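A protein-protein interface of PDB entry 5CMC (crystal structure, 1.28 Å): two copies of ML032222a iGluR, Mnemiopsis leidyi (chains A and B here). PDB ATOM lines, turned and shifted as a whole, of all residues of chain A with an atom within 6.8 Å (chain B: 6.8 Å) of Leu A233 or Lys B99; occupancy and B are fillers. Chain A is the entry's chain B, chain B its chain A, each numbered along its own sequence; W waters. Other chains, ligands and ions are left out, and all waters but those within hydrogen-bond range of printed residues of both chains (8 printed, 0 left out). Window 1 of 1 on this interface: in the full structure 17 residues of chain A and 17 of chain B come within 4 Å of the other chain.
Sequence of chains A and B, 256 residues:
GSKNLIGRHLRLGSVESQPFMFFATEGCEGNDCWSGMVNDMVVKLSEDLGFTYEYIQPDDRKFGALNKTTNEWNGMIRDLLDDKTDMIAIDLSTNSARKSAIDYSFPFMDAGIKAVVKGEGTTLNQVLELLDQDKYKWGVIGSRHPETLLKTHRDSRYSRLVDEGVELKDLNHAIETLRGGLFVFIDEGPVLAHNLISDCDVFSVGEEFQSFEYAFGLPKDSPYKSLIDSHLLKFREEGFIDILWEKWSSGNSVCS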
ATOM      1  N   PHE A 106       6.070  -2.283 -20.542  1.00  0.00           N
ATOM      2  CA  PHE A 106       7.039  -1.757 -21.476  1.00  0.00           C
ATOM      3  C   PHE A 106       6.296  -0.900 -22.497  1.00  0.00           C
ATOM      4  O   PHE A 106       5.177  -1.219 -22.897  1.00  0.00           O
ATOM      5  CB  PHE A 106       7.780  -2.895 -22.175  1.00  0.00           C
ATOM      6  CG  PHE A 106       9.053  -2.448 -22.810  1.00  0.00           C
ATOM      7  CD1 PHE A 106      10.237  -2.359 -22.088  1.00  0.00           C
ATOM      8  CD2 PHE A 106       9.047  -2.043 -24.138  1.00  0.00           C
ATOM      9  CE1 PHE A 106      11.403  -1.905 -22.688  1.00  0.00           C
ATOM     10  CE2 PHE A 106      10.198  -1.580 -24.739  1.00  0.00           C
ATOM     11  CZ  PHE A 106      11.380  -1.506 -24.007  1.00  0.00           C
ATOM     12  N   PRO A 107       6.885   0.221 -22.902  1.00  0.00           N
ATOM     13  CA  PRO A 107       6.174   1.113 -23.827  1.00  0.00           C
ATOM     14  C   PRO A 107       6.108   0.574 -25.243  1.00  0.00           C
ATOM     15  O   PRO A 107       7.058  -0.070 -25.696  1.00  0.00           O
ATOM     16  CB  PRO A 107       7.022   2.384 -23.785  1.00  0.00           C
ATOM     17  CG  PRO A 107       8.350   1.933 -23.388  1.00  0.00           C
ATOM     18  CD  PRO A 107       8.160   0.795 -22.448  1.00  0.00           C
ATOM     19  N   SER A 226       5.739  -9.312 -16.159  1.00  0.00           N
ATOM     20  CA  SER A 226       6.993  -9.716 -16.781  1.00  0.00           C
ATOM     21  C   SER A 226       6.754 -10.252 -18.187  1.00  0.00           C
ATOM     22  O   SER A 226       7.448  -9.882 -19.126  1.00  0.00           O
ATOM     23  CB  SER A 226       7.741 -10.762 -15.935  1.00  0.00           C
ATOM     24  OG  SER A 226       8.966 -11.142 -16.548  1.00  0.00           O
ATOM     25  N   ILE A 228       4.012  -9.832 -20.146  1.00  0.00           N
ATOM     26  CA  ILE A 228       3.491  -8.806 -21.035  1.00  0.00           C
ATOM     27  C   ILE A 228       4.631  -7.911 -21.520  1.00  0.00           C
ATOM     28  O   ILE A 228       4.738  -7.616 -22.715  1.00  0.00           O
ATOM     29  CB  ILE A 228       2.384  -7.999 -20.343  1.00  0.00           C
ATOM     30  CG1 ILE A 228       1.131  -8.875 -20.127  1.00  0.00           C
ATOM     31  CG2 ILE A 228       2.054  -6.728 -21.129  1.00  0.00           C
ATOM     32  CD1 ILE A 228       0.421  -9.294 -21.391  1.00  0.00           C
ATOM     33  N   ASP A 229       5.501  -7.504 -20.597  1.00  0.00           N
ATOM     34  CA  ASP A 229       6.620  -6.654 -20.977  1.00  0.00           C
ATOM     35  C   ASP A 229       7.536  -7.299 -22.008  1.00  0.00           C
ATOM     36  O   ASP A 229       7.941  -6.657 -22.972  1.00  0.00           O
ATOM     37  CB  ASP A 229       7.467  -6.311 -19.767  1.00  0.00           C
ATOM     38  CG  ASP A 229       6.807  -5.308 -18.831  1.00  0.00           C
ATOM     39  OD1 ASP A 229       5.765  -4.728 -19.188  1.00  0.00           O
ATOM     40  OD2 ASP A 229       7.362  -5.082 -17.726  1.00  0.00           O
ATOM     41  N   SER A 230       7.906  -8.555 -21.774  1.00  0.00           N
ATOM     42  CA  SER A 230       8.795  -9.241 -22.703  1.00  0.00           C
ATOM     43  C   SER A 230       8.176  -9.266 -24.097  1.00  0.00           C
ATOM     44  O   SER A 230       8.813  -8.938 -25.085  1.00  0.00           O
ATOM     45  CB  SER A 230       9.073 -10.661 -22.232  1.00  0.00           C
ATOM     46  OG  SER A 230       9.873 -10.644 -21.066  1.00  0.00           O
ATOM     47  N   HIS A 231       6.898  -9.627 -24.166  1.00  0.00           N
ATOM     48  CA  HIS A 231       6.230  -9.754 -25.442  1.00  0.00           C
ATOM     49  C   HIS A 231       6.048  -8.415 -26.136  1.00  0.00           C
ATOM     50  O   HIS A 231       6.207  -8.330 -27.346  1.00  0.00           O
ATOM     51  CB  HIS A 231       4.936 -10.554 -25.312  1.00  0.00           C
ATOM     52  CG  HIS A 231       5.193 -12.014 -25.099  1.00  0.00           C
ATOM     53  ND1 HIS A 231       4.867 -12.972 -26.030  1.00  0.00           N
ATOM     54  CD2 HIS A 231       5.837 -12.664 -24.101  1.00  0.00           C
ATOM     55  CE1 HIS A 231       5.263 -14.156 -25.599  1.00  0.00           C
ATOM     56  NE2 HIS A 231       5.878 -13.994 -24.443  1.00  0.00           N
ATOM     57  N   LEU A 232       5.750  -7.359 -25.380  1.00  0.00           N
ATOM     58  CA  LEU A 232       5.626  -6.044 -26.008  1.00  0.00           C
ATOM     59  C   LEU A 232       6.971  -5.558 -26.526  1.00  0.00           C
ATOM     60  O   LEU A 232       7.038  -4.950 -27.588  1.00  0.00           O
ATOM     61  CB  LEU A 232       5.033  -5.017 -25.060  1.00  0.00           C
ATOM     62  CG  LEU A 232       3.542  -5.195 -24.753  1.00  0.00           C
ATOM     63  CD1 LEU A 232       3.141  -4.196 -23.731  1.00  0.00           C
ATOM     64  CD2 LEU A 232       2.695  -5.049 -25.999  1.00  0.00           C
ATOM     65  N   LEU A 233       8.041  -5.805 -25.775  1.00  0.00           N
ATOM     66  CA  LEU A 233       9.376  -5.442 -26.249  1.00  0.00           C
ATOM     67  C   LEU A 233       9.694  -6.177 -27.550  1.00  0.00           C
ATOM     68  O   LEU A 233      10.208  -5.585 -28.493  1.00  0.00           O
ATOM     69  CB  LEU A 233      10.411  -5.729 -25.173  1.00  0.00           C
ATOM     70  CG  LEU A 233      11.872  -5.511 -25.548  1.00  0.00           C
ATOM     71  CD1 LEU A 233      12.156  -4.145 -26.150  1.00  0.00           C
ATOM     72  CD2 LEU A 233      12.734  -5.780 -24.330  1.00  0.00           C
ATOM     73  N   LYS A 234       9.375  -7.464 -27.619  1.00  0.00           N
ATOM     74  CA  LYS A 234       9.581  -8.216 -28.853  1.00  0.00           C
ATOM     75  C   LYS A 234       8.766  -7.642 -30.018  1.00  0.00           C
ATOM     76  O   LYS A 234       9.282  -7.483 -31.110  1.00  0.00           O
ATOM     77  CB  LYS A 234       9.200  -9.680 -28.614  1.00  0.00           C
ATOM     78  CG  LYS A 234       9.796 -10.646 -29.599  1.00  0.00           C
ATOM     79  CD  LYS A 234      11.277 -10.891 -29.271  1.00  0.00           C
ATOM     80  CE  LYS A 234      11.851 -12.083 -30.038  1.00  0.00           C
ATOM     81  NZ  LYS A 234      13.198 -12.488 -29.533  1.00  0.00           N
ATOM     82  N   PHE A 235       7.503  -7.289 -29.771  1.00  0.00           N
ATOM     83  CA  PHE A 235       6.691  -6.680 -30.815  1.00  0.00           C
ATOM     84  C   PHE A 235       7.402  -5.448 -31.355  1.00  0.00           C
ATOM     85  O   PHE A 235       7.476  -5.224 -32.560  1.00  0.00           O
ATOM     86  CB  PHE A 235       5.335  -6.206 -30.293  1.00  0.00           C
ATOM     87  CG  PHE A 235       4.307  -7.288 -30.034  1.00  0.00           C
ATOM     88  CD1 PHE A 235       4.485  -8.619 -30.366  1.00  0.00           C
ATOM     89  CD2 PHE A 235       3.105  -6.909 -29.470  1.00  0.00           C
ATOM     90  CE1 PHE A 235       3.482  -9.544 -30.111  1.00  0.00           C
ATOM     91  CE2 PHE A 235       2.120  -7.814 -29.218  1.00  0.00           C
ATOM     92  CZ  PHE A 235       2.303  -9.130 -29.525  1.00  0.00           C
ATOM     93  N   ARG A 236       7.913  -4.624 -30.450  1.00  0.00           N
ATOM     94  CA  ARG A 236       8.555  -3.388 -30.866  1.00  0.00           C
ATOM     95  C   ARG A 236       9.837  -3.656 -31.642  1.00  0.00           C
ATOM     96  O   ARG A 236      10.040  -3.133 -32.719  1.00  0.00           O
ATOM     97  CB  ARG A 236       8.810  -2.512 -29.644  1.00  0.00           C
ATOM     98  CG  ARG A 236       9.071  -1.087 -30.016  1.00  0.00           C
ATOM     99  CD  ARG A 236       8.861  -0.189 -28.848  1.00  0.00           C
ATOM    100  NE  ARG A 236       9.172   1.186 -29.189  1.00  0.00           N
ATOM    101  CZ  ARG A 236       9.502   2.110 -28.296  1.00  0.00           C
ATOM    102  NH1 ARG A 236       9.542   1.808 -27.001  1.00  0.00           N
ATOM    103  NH2 ARG A 236       9.787   3.339 -28.699  1.00  0.00           N
ATOM    104  N   GLU A 237      10.682  -4.515 -31.095  1.00  0.00           N
ATOM    105  CA  GLU A 237      11.962  -4.809 -31.686  1.00  0.00           C
ATOM    106  C   GLU A 237      11.819  -5.465 -33.058  1.00  0.00           C
ATOM    107  O   GLU A 237      12.628  -5.219 -33.960  1.00  0.00           O
ATOM    108  CB  GLU A 237      12.728  -5.715 -30.728  1.00  0.00           C
ATOM    109  CG  GLU A 237      14.140  -6.026 -31.144  1.00  0.00           C
ATOM    110  CD  GLU A 237      14.914  -6.735 -30.046  1.00  0.00           C
ATOM    111  OE1 GLU A 237      15.132  -6.164 -28.972  1.00  0.00           O
ATOM    112  OE2 GLU A 237      15.307  -7.893 -30.241  1.00  0.00           O
ATOM    113  N   GLU A 238      10.793  -6.293 -33.224  1.00  0.00           N
ATOM    114  CA  GLU A 238      10.550  -6.991 -34.481  1.00  0.00           C
ATOM    115  C   GLU A 238       9.888  -6.121 -35.530  1.00  0.00           C
ATOM    116  O   GLU A 238       9.753  -6.547 -36.674  1.00  0.00           O
ATOM    117  CB  GLU A 238       9.702  -8.267 -34.254  1.00  0.00           C
ATOM    118  CG  GLU A 238      10.468  -9.343 -33.508  1.00  0.00           C
ATOM    119  CD  GLU A 238       9.666 -10.602 -33.216  1.00  0.00           C
ATOM    120  OE1 GLU A 238       8.424 -10.525 -33.171  1.00  0.00           O
ATOM    121  OE2 GLU A 238      10.307 -11.665 -33.016  1.00  0.00           O
ATOM    122  N   GLY A 239       9.452  -4.924 -35.162  1.00  0.00           N
ATOM    123  CA  GLY A 239       8.817  -4.019 -36.102  1.00  0.00           C
ATOM    124  C   GLY A 239       7.318  -4.156 -36.216  1.00  0.00           C
ATOM    125  O   GLY A 239       6.710  -3.511 -37.061  1.00  0.00           O
ATOM    126  N   TRP B  73      26.610 -14.606 -20.342  1.00  0.00           N
ATOM    127  CA  TRP B  73      26.694 -13.161 -20.488  1.00  0.00           C
ATOM    128  C   TRP B  73      28.073 -12.640 -20.134  1.00  0.00           C
ATOM    129  O   TRP B  73      28.821 -13.285 -19.388  1.00  0.00           O
ATOM    130  CB  TRP B  73      25.682 -12.494 -19.552  1.00  0.00           C
ATOM    131  CG  TRP B  73      24.279 -12.650 -20.036  1.00  0.00           C
ATOM    132  CD1 TRP B  73      23.400 -13.639 -19.709  1.00  0.00           C
ATOM    133  CD2 TRP B  73      23.592 -11.793 -20.960  1.00  0.00           C
ATOM    134  NE1 TRP B  73      22.208 -13.443 -20.360  1.00  0.00           N
ATOM    135  CE2 TRP B  73      22.298 -12.319 -21.138  1.00  0.00           C
ATOM    136  CE3 TRP B  73      23.947 -10.623 -21.649  1.00  0.00           C
ATOM    137  CZ2 TRP B  73      21.355 -11.713 -21.979  1.00  0.00           C
ATOM    138  CZ3 TRP B  73      23.028 -10.033 -22.489  1.00  0.00           C
ATOM    139  CH2 TRP B  73      21.741 -10.574 -22.648  1.00  0.00           C
ATOM    140  N   THR B  94      17.451  -1.082 -24.529  1.00  0.00           N
ATOM    141  CA  THR B  94      16.461  -2.147 -24.358  1.00  0.00           C
ATOM    142  C   THR B  94      16.510  -3.110 -25.537  1.00  0.00           C
ATOM    143  O   THR B  94      16.376  -2.702 -26.691  1.00  0.00           O
ATOM    144  CB  THR B  94      15.040  -1.587 -24.166  1.00  0.00           C
ATOM    145  OG1 THR B  94      14.761  -0.686 -25.238  1.00  0.00           O
ATOM    146  CG2 THR B  94      14.941  -0.871 -22.826  1.00  0.00           C
ATOM    147  N   ASN B  95      16.721  -4.388 -25.250  1.00  0.00           N
ATOM    148  CA  ASN B  95      16.618  -5.437 -26.269  1.00  0.00           C
ATOM    149  C   ASN B  95      16.136  -6.733 -25.649  1.00  0.00           C
ATOM    150  O   ASN B  95      16.203  -6.911 -24.437  1.00  0.00           O
ATOM    151  CB  ASN B  95      17.910  -5.610 -27.116  1.00  0.00           C
ATOM    152  CG  ASN B  95      19.096  -6.193 -26.343  1.00  0.00           C
ATOM    153  OD1 ASN B  95      19.005  -7.238 -25.723  1.00  0.00           O
ATOM    154  ND2 ASN B  95      20.241  -5.524 -26.440  1.00  0.00           N
ATOM    155  N   SER B  96      15.569  -7.600 -26.488  1.00  0.00           N
ATOM    156  CA  SER B  96      14.922  -8.804 -26.002  1.00  0.00           C
ATOM    157  C   SER B  96      15.914  -9.773 -25.355  1.00  0.00           C
ATOM    158  O   SER B  96      15.561 -10.486 -24.423  1.00  0.00           O
ATOM    159  CB  SER B  96      14.142  -9.507 -27.111  1.00  0.00           C
ATOM    160  OG  SER B  96      13.035  -8.734 -27.546  1.00  0.00           O
ATOM    161  N   ALA B  97      17.139  -9.844 -25.870  1.00  0.00           N
ATOM    162  CA  ALA B  97      18.130 -10.737 -25.258  1.00  0.00           C
ATOM    163  C   ALA B  97      18.349 -10.359 -23.781  1.00  0.00           C
ATOM    164  O   ALA B  97      18.270 -11.195 -22.877  1.00  0.00           O
ATOM    165  CB  ALA B  97      19.445 -10.695 -26.028  1.00  0.00           C
ATOM    166  N   ARG B  98      18.584  -9.085 -23.531  1.00  0.00           N
ATOM    167  CA  ARG B  98      18.806  -8.638 -22.164  1.00  0.00           C
ATOM    168  C   ARG B  98      17.560  -8.840 -21.311  1.00  0.00           C
ATOM    169  O   ARG B  98      17.654  -9.245 -20.153  1.00  0.00           O
ATOM    170  CB  ARG B  98      19.256  -7.178 -22.130  1.00  0.00           C
ATOM    171  CG  ARG B  98      20.656  -6.971 -22.686  1.00  0.00           C
ATOM    172  CD  ARG B  98      20.959  -5.522 -22.915  1.00  0.00           C
ATOM    173  NE  ARG B  98      22.364  -5.344 -23.302  1.00  0.00           N
ATOM    174  CZ  ARG B  98      22.890  -4.190 -23.712  1.00  0.00           C
ATOM    175  NH1 ARG B  98      22.136  -3.098 -23.769  1.00  0.00           N
ATOM    176  NH2 ARG B  98      24.188  -4.110 -24.003  1.00  0.00           N
ATOM    177  N   LYS B  99      16.390  -8.564 -21.881  1.00  0.00           N
ATOM    178  CA  LYS B  99      15.144  -8.686 -21.139  1.00  0.00           C
ATOM    179  C   LYS B  99      14.930 -10.130 -20.658  1.00  0.00           C
ATOM    180  O   LYS B  99      14.293 -10.353 -19.627  1.00  0.00           O
ATOM    181  CB  LYS B  99      13.981  -8.223 -22.022  1.00  0.00           C
ATOM    182  CG  LYS B  99      12.570  -8.417 -21.451  1.00  0.00           C
ATOM    183  CD  LYS B  99      12.093  -7.247 -20.614  1.00  0.00           C
ATOM    184  CE  LYS B  99      12.727  -7.184 -19.245  1.00  0.00           C
ATOM    185  NZ  LYS B  99      12.618  -8.447 -18.469  1.00  0.00           N
ATOM    186  N   SER B 100      15.470 -11.111 -21.379  1.00  0.00           N
ATOM    187  CA  SER B 100      15.313 -12.497 -20.959  1.00  0.00           C
ATOM    188  C   SER B 100      16.075 -12.786 -19.663  1.00  0.00           C
ATOM    189  O   SER B 100      15.801 -13.784 -18.993  1.00  0.00           O
ATOM    190  CB  SER B 100      15.775 -13.443 -22.076  1.00  0.00           C
ATOM    191  OG  SER B 100      17.193 -13.519 -22.152  1.00  0.00           O
ATOM    192  N   ALA B 101      17.021 -11.912 -19.309  1.00  0.00           N
ATOM    193  CA  ALA B 101      17.866 -12.123 -18.116  1.00  0.00           C
ATOM    194  C   ALA B 101      17.679 -11.092 -17.005  1.00  0.00           C
ATOM    195  O   ALA B 101      17.859 -11.411 -15.830  1.00  0.00           O
ATOM    196  CB  ALA B 101      19.319 -12.158 -18.538  1.00  0.00           C
ATOM    197  N   ILE B 102      17.368  -9.858 -17.381  1.00  0.00           N
ATOM    198  CA  ILE B 102      17.256  -8.755 -16.427  1.00  0.00           C
ATOM    199  C   ILE B 102      16.002  -7.951 -16.707  1.00  0.00           C
ATOM    200  O   ILE B 102      15.369  -8.119 -17.739  1.00  0.00           O
ATOM    201  CB  ILE B 102      18.498  -7.788 -16.454  1.00  0.00           C
ATOM    202  CG1 ILE B 102      18.605  -7.011 -17.779  1.00  0.00           C
ATOM    203  CG2 ILE B 102      19.775  -8.569 -16.159  1.00  0.00           C
ATOM    204  CD1 ILE B 102      19.414  -5.729 -17.665  1.00  0.00           C
ATOM    205  N   ASP B 103      15.668  -7.071 -15.768  1.00  0.00           N
ATOM    206  CA  ASP B 103      14.635  -6.070 -15.967  1.00  0.00           C
ATOM    207  C   ASP B 103      15.285  -4.740 -16.324  1.00  0.00           C
ATOM    208  O   ASP B 103      16.491  -4.531 -16.163  1.00  0.00           O
ATOM    209  CB  ASP B 103      13.776  -5.893 -14.712  1.00  0.00           C
ATOM    210  CG  ASP B 103      12.763  -6.987 -14.521  1.00  0.00           C
ATOM    211  OD1 ASP B 103      12.545  -7.806 -15.440  1.00  0.00           O
ATOM    212  OD2 ASP B 103      12.134  -6.993 -13.448  1.00  0.00           O
ATOM    213  N   TYR B 104      14.449  -3.841 -16.824  1.00  0.00           N
ATOM    214  CA  TYR B 104      14.822  -2.471 -17.070  1.00  0.00           C
ATOM    215  C   TYR B 104      14.011  -1.541 -16.208  1.00  0.00           C
ATOM    216  O   TYR B 104      12.866  -1.835 -15.847  1.00  0.00           O
ATOM    217  CB  TYR B 104      14.560  -2.105 -18.512  1.00  0.00           C
ATOM    218  CG  TYR B 104      15.500  -2.740 -19.518  1.00  0.00           C
ATOM    219  CD1 TYR B 104      16.710  -2.148 -19.800  1.00  0.00           C
ATOM    220  CD2 TYR B 104      15.165  -3.901 -20.203  1.00  0.00           C
ATOM    221  CE1 TYR B 104      17.559  -2.668 -20.734  1.00  0.00           C
ATOM    222  CE2 TYR B 104      16.016  -4.455 -21.145  1.00  0.00           C
ATOM    223  CZ  TYR B 104      17.211  -3.832 -21.401  1.00  0.00           C
ATOM    224  OH  TYR B 104      18.045  -4.327 -22.369  1.00  0.00           O
ATOM    225  N   SER B 211      13.600   0.971 -33.138  1.00  0.00           N
ATOM    226  CA  SER B 211      13.219   1.950 -32.110  1.00  0.00           C
ATOM    227  C   SER B 211      13.335   1.313 -30.723  1.00  0.00           C
ATOM    228  O   SER B 211      12.779   0.226 -30.495  1.00  0.00           O
ATOM    229  CB  SER B 211      11.785   2.418 -32.358  1.00  0.00           C
ATOM    230  OG  SER B 211      11.484   3.584 -31.615  1.00  0.00           O
ATOM    231  N   PHE B 212      14.076   1.946 -29.803  1.00  0.00           N
ATOM    232  CA  PHE B 212      14.260   1.390 -28.468  1.00  0.00           C
ATOM    233  C   PHE B 212      14.477   2.530 -27.489  1.00  0.00           C
ATOM    234  O   PHE B 212      14.298   3.707 -27.828  1.00  0.00           O
ATOM    235  CB  PHE B 212      15.396   0.349 -28.470  1.00  0.00           C
ATOM    236  CG  PHE B 212      16.705   0.879 -28.988  1.00  0.00           C
ATOM    237  CD1 PHE B 212      16.989   0.834 -30.350  1.00  0.00           C
ATOM    238  CD2 PHE B 212      17.648   1.437 -28.116  1.00  0.00           C
ATOM    239  CE1 PHE B 212      18.189   1.335 -30.832  1.00  0.00           C
ATOM    240  CE2 PHE B 212      18.850   1.936 -28.608  1.00  0.00           C
ATOM    241  CZ  PHE B 212      19.111   1.896 -29.966  1.00  0.00           C
ATOM    242  N   LYS B 220      16.020  -9.021 -11.800  1.00  0.00           N
ATOM    243  CA  LYS B 220      14.644  -9.446 -11.608  1.00  0.00           C
ATOM    244  C   LYS B 220      14.334  -9.481 -10.104  1.00  0.00           C
ATOM    245  O   LYS B 220      15.189  -9.823  -9.288  1.00  0.00           O
ATOM    246  CB  LYS B 220      14.404 -10.795 -12.278  1.00  0.00           C
ATOM    247  CG  LYS B 220      14.413 -10.709 -13.790  1.00  0.00           C
ATOM    248  CD  LYS B 220      14.200 -12.059 -14.420  1.00  0.00           C
ATOM    249  CE  LYS B 220      13.984 -11.934 -15.916  1.00  0.00           C
ATOM    250  NZ  LYS B 220      13.568 -13.220 -16.546  1.00  0.00           N
HETATM  251  O   HOH W   1      11.903  -1.215 -34.006  1.00  0.00           O
HETATM  252  O   HOH W   2      12.358   4.987 -29.407  1.00  0.00           O
HETATM  253  O   HOH W   3      11.632  -9.241 -25.123  1.00  0.00           O
HETATM  254  O   HOH W   4       9.907  -8.764 -18.243  1.00  0.00           O
HETATM  255  O   HOH W   5      12.141 -12.070 -18.835  1.00  0.00           O
HETATM  256  O   HOH W   6      17.545  -8.970 -28.871  1.00  0.00           O
HETATM  257  O   HOH W   7      14.904  -3.389 -28.967  1.00  0.00           O
HETATM  258  O   HOH W   8      10.887 -10.003 -15.157  1.00  0.00           O
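The backbone NH of Ser B96 lies within hydrogen-bond range of the side-chain carboxylate of Glu A237 (2.9 Å).
The side-chain hydroxyl (OG) of Ser B211 is in hydrogen-bond range of the guanidinium group (NH2) of Arg A236, 3.4 Å away.
The side-chain amide oxygen (OD1) of Asn B95 lies within hydrogen-bond range of the backbone NH (N) of Arg B98, 2.9 Å away.
N of Phe A106 lies within hydrogen-bond range of OD1 of Asp A229 (2.8 Å).
The side-chain amide oxygen (OD1) of Asn B95 sits at hydrogen-bond distance from the backbone NH (N) of Ala B97 (3.2 Å).
The side-chain amino group (NZ) of Lys B99 is in hydrogen-bond range of the backbone carbonyl oxygen (O) of Ile B102.
NH1 of Arg A236 lies within hydrogen-bond range of O of Pro A107 (3.4 Å).
The side-chain amino group (NZ) of Lys B99 lies within salt-bridge range of the side-chain carboxylate (OD1) of Asp B103 (3.1 Å).
Among the printed residues, pairs that only touch across the chains: Phe A106 with Thr B94 (3.7 Å), Ser A230 with Lys B99 (3.5 Å), Leu A233 with Asn B95 (3.7 Å), Leu A233 with Ser B96 (3.97 Å), Leu A233 with Lys B99 (3.6 Å), Lys A234 with Ser B96 (3.3 Å) and Glu A237 with Asn B95 (3.2 Å).
Printed residues of chain B within 4 Å of Phe A106: Thr B94 (3.7 Å).
Printed residues of chain B within 4 Å of Leu A233: Asn B95 (3.7 Å), Ser B96 (3.97 Å) and Lys B99 (3.6 Å).
Of the printed residues of chain B, Lys A234 touches Ser B96 (3.3 Å).
Of the printed residues of chain B, Arg A236 touches Ser B211 (3.4 Å).
Of the printed residues of chain A, Lys B99 touches Ser A230 and Leu A233.
Ala B101 touches none of the printed residues of chain A.
Printed residues of chain A within 4 Å of Ser B211: Arg A236 (3.4 Å).
The nearest printed residue of chain A that does not touch Lys B99 is Asp A229 (4.8 Å).
The nearest printed residue of chain A that does not touch Thr B94 is Glu A237 (4.3 Å).
Of the 15 printed residues of chain B, 5 touch a printed residue of chain A.
Printed residues of chain B that touch a printed residue of chain A: Thr B94, Asn B95, Ser B96, Lys B99 and Ser B211.
Hydrophobic or aromatic side chains of chain A within 4 Å of the printed part of chain B: Phe A106 and Leu A233.
Among the printed residues, 9 pairs touch across the chains.
Among the printed residues, no Asp or Glu carboxylate lies within 4 Å of a Lys or Arg side-chain nitrogen of the other chain.
No position is printed for both chains.
Water W8 lies within hydrogen-bond range of OG of Ser A226 (2.6 Å) and OD1 of Asp B103 (2.8 Å).
Water W4 lies within hydrogen-bond range of NZ of Lys B99 (2.7 Å), O of Ser A226 (2.8 Å) and OG of Ser A230 (3.4 Å).
Water W2 lies within hydrogen-bond range of OG of Ser B211 (2.8 Å), O of Phe B212 (2.8 Å) and NH2 of Arg A236 (3.1 Å).
Water W3 lies within hydrogen-bond range of O of Ser A230 (2.8 Å) and OG of Ser B96 (2.8 Å).
Water W6 lies within hydrogen-bond range of OE2 of Glu A237 (2.8 Å), N of Ala B97 (3.2 Å) and N of Ser B96 (3.4 Å).
Water W1 lies within hydrogen-bond range of N of Ser B211 and O of Arg A236.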
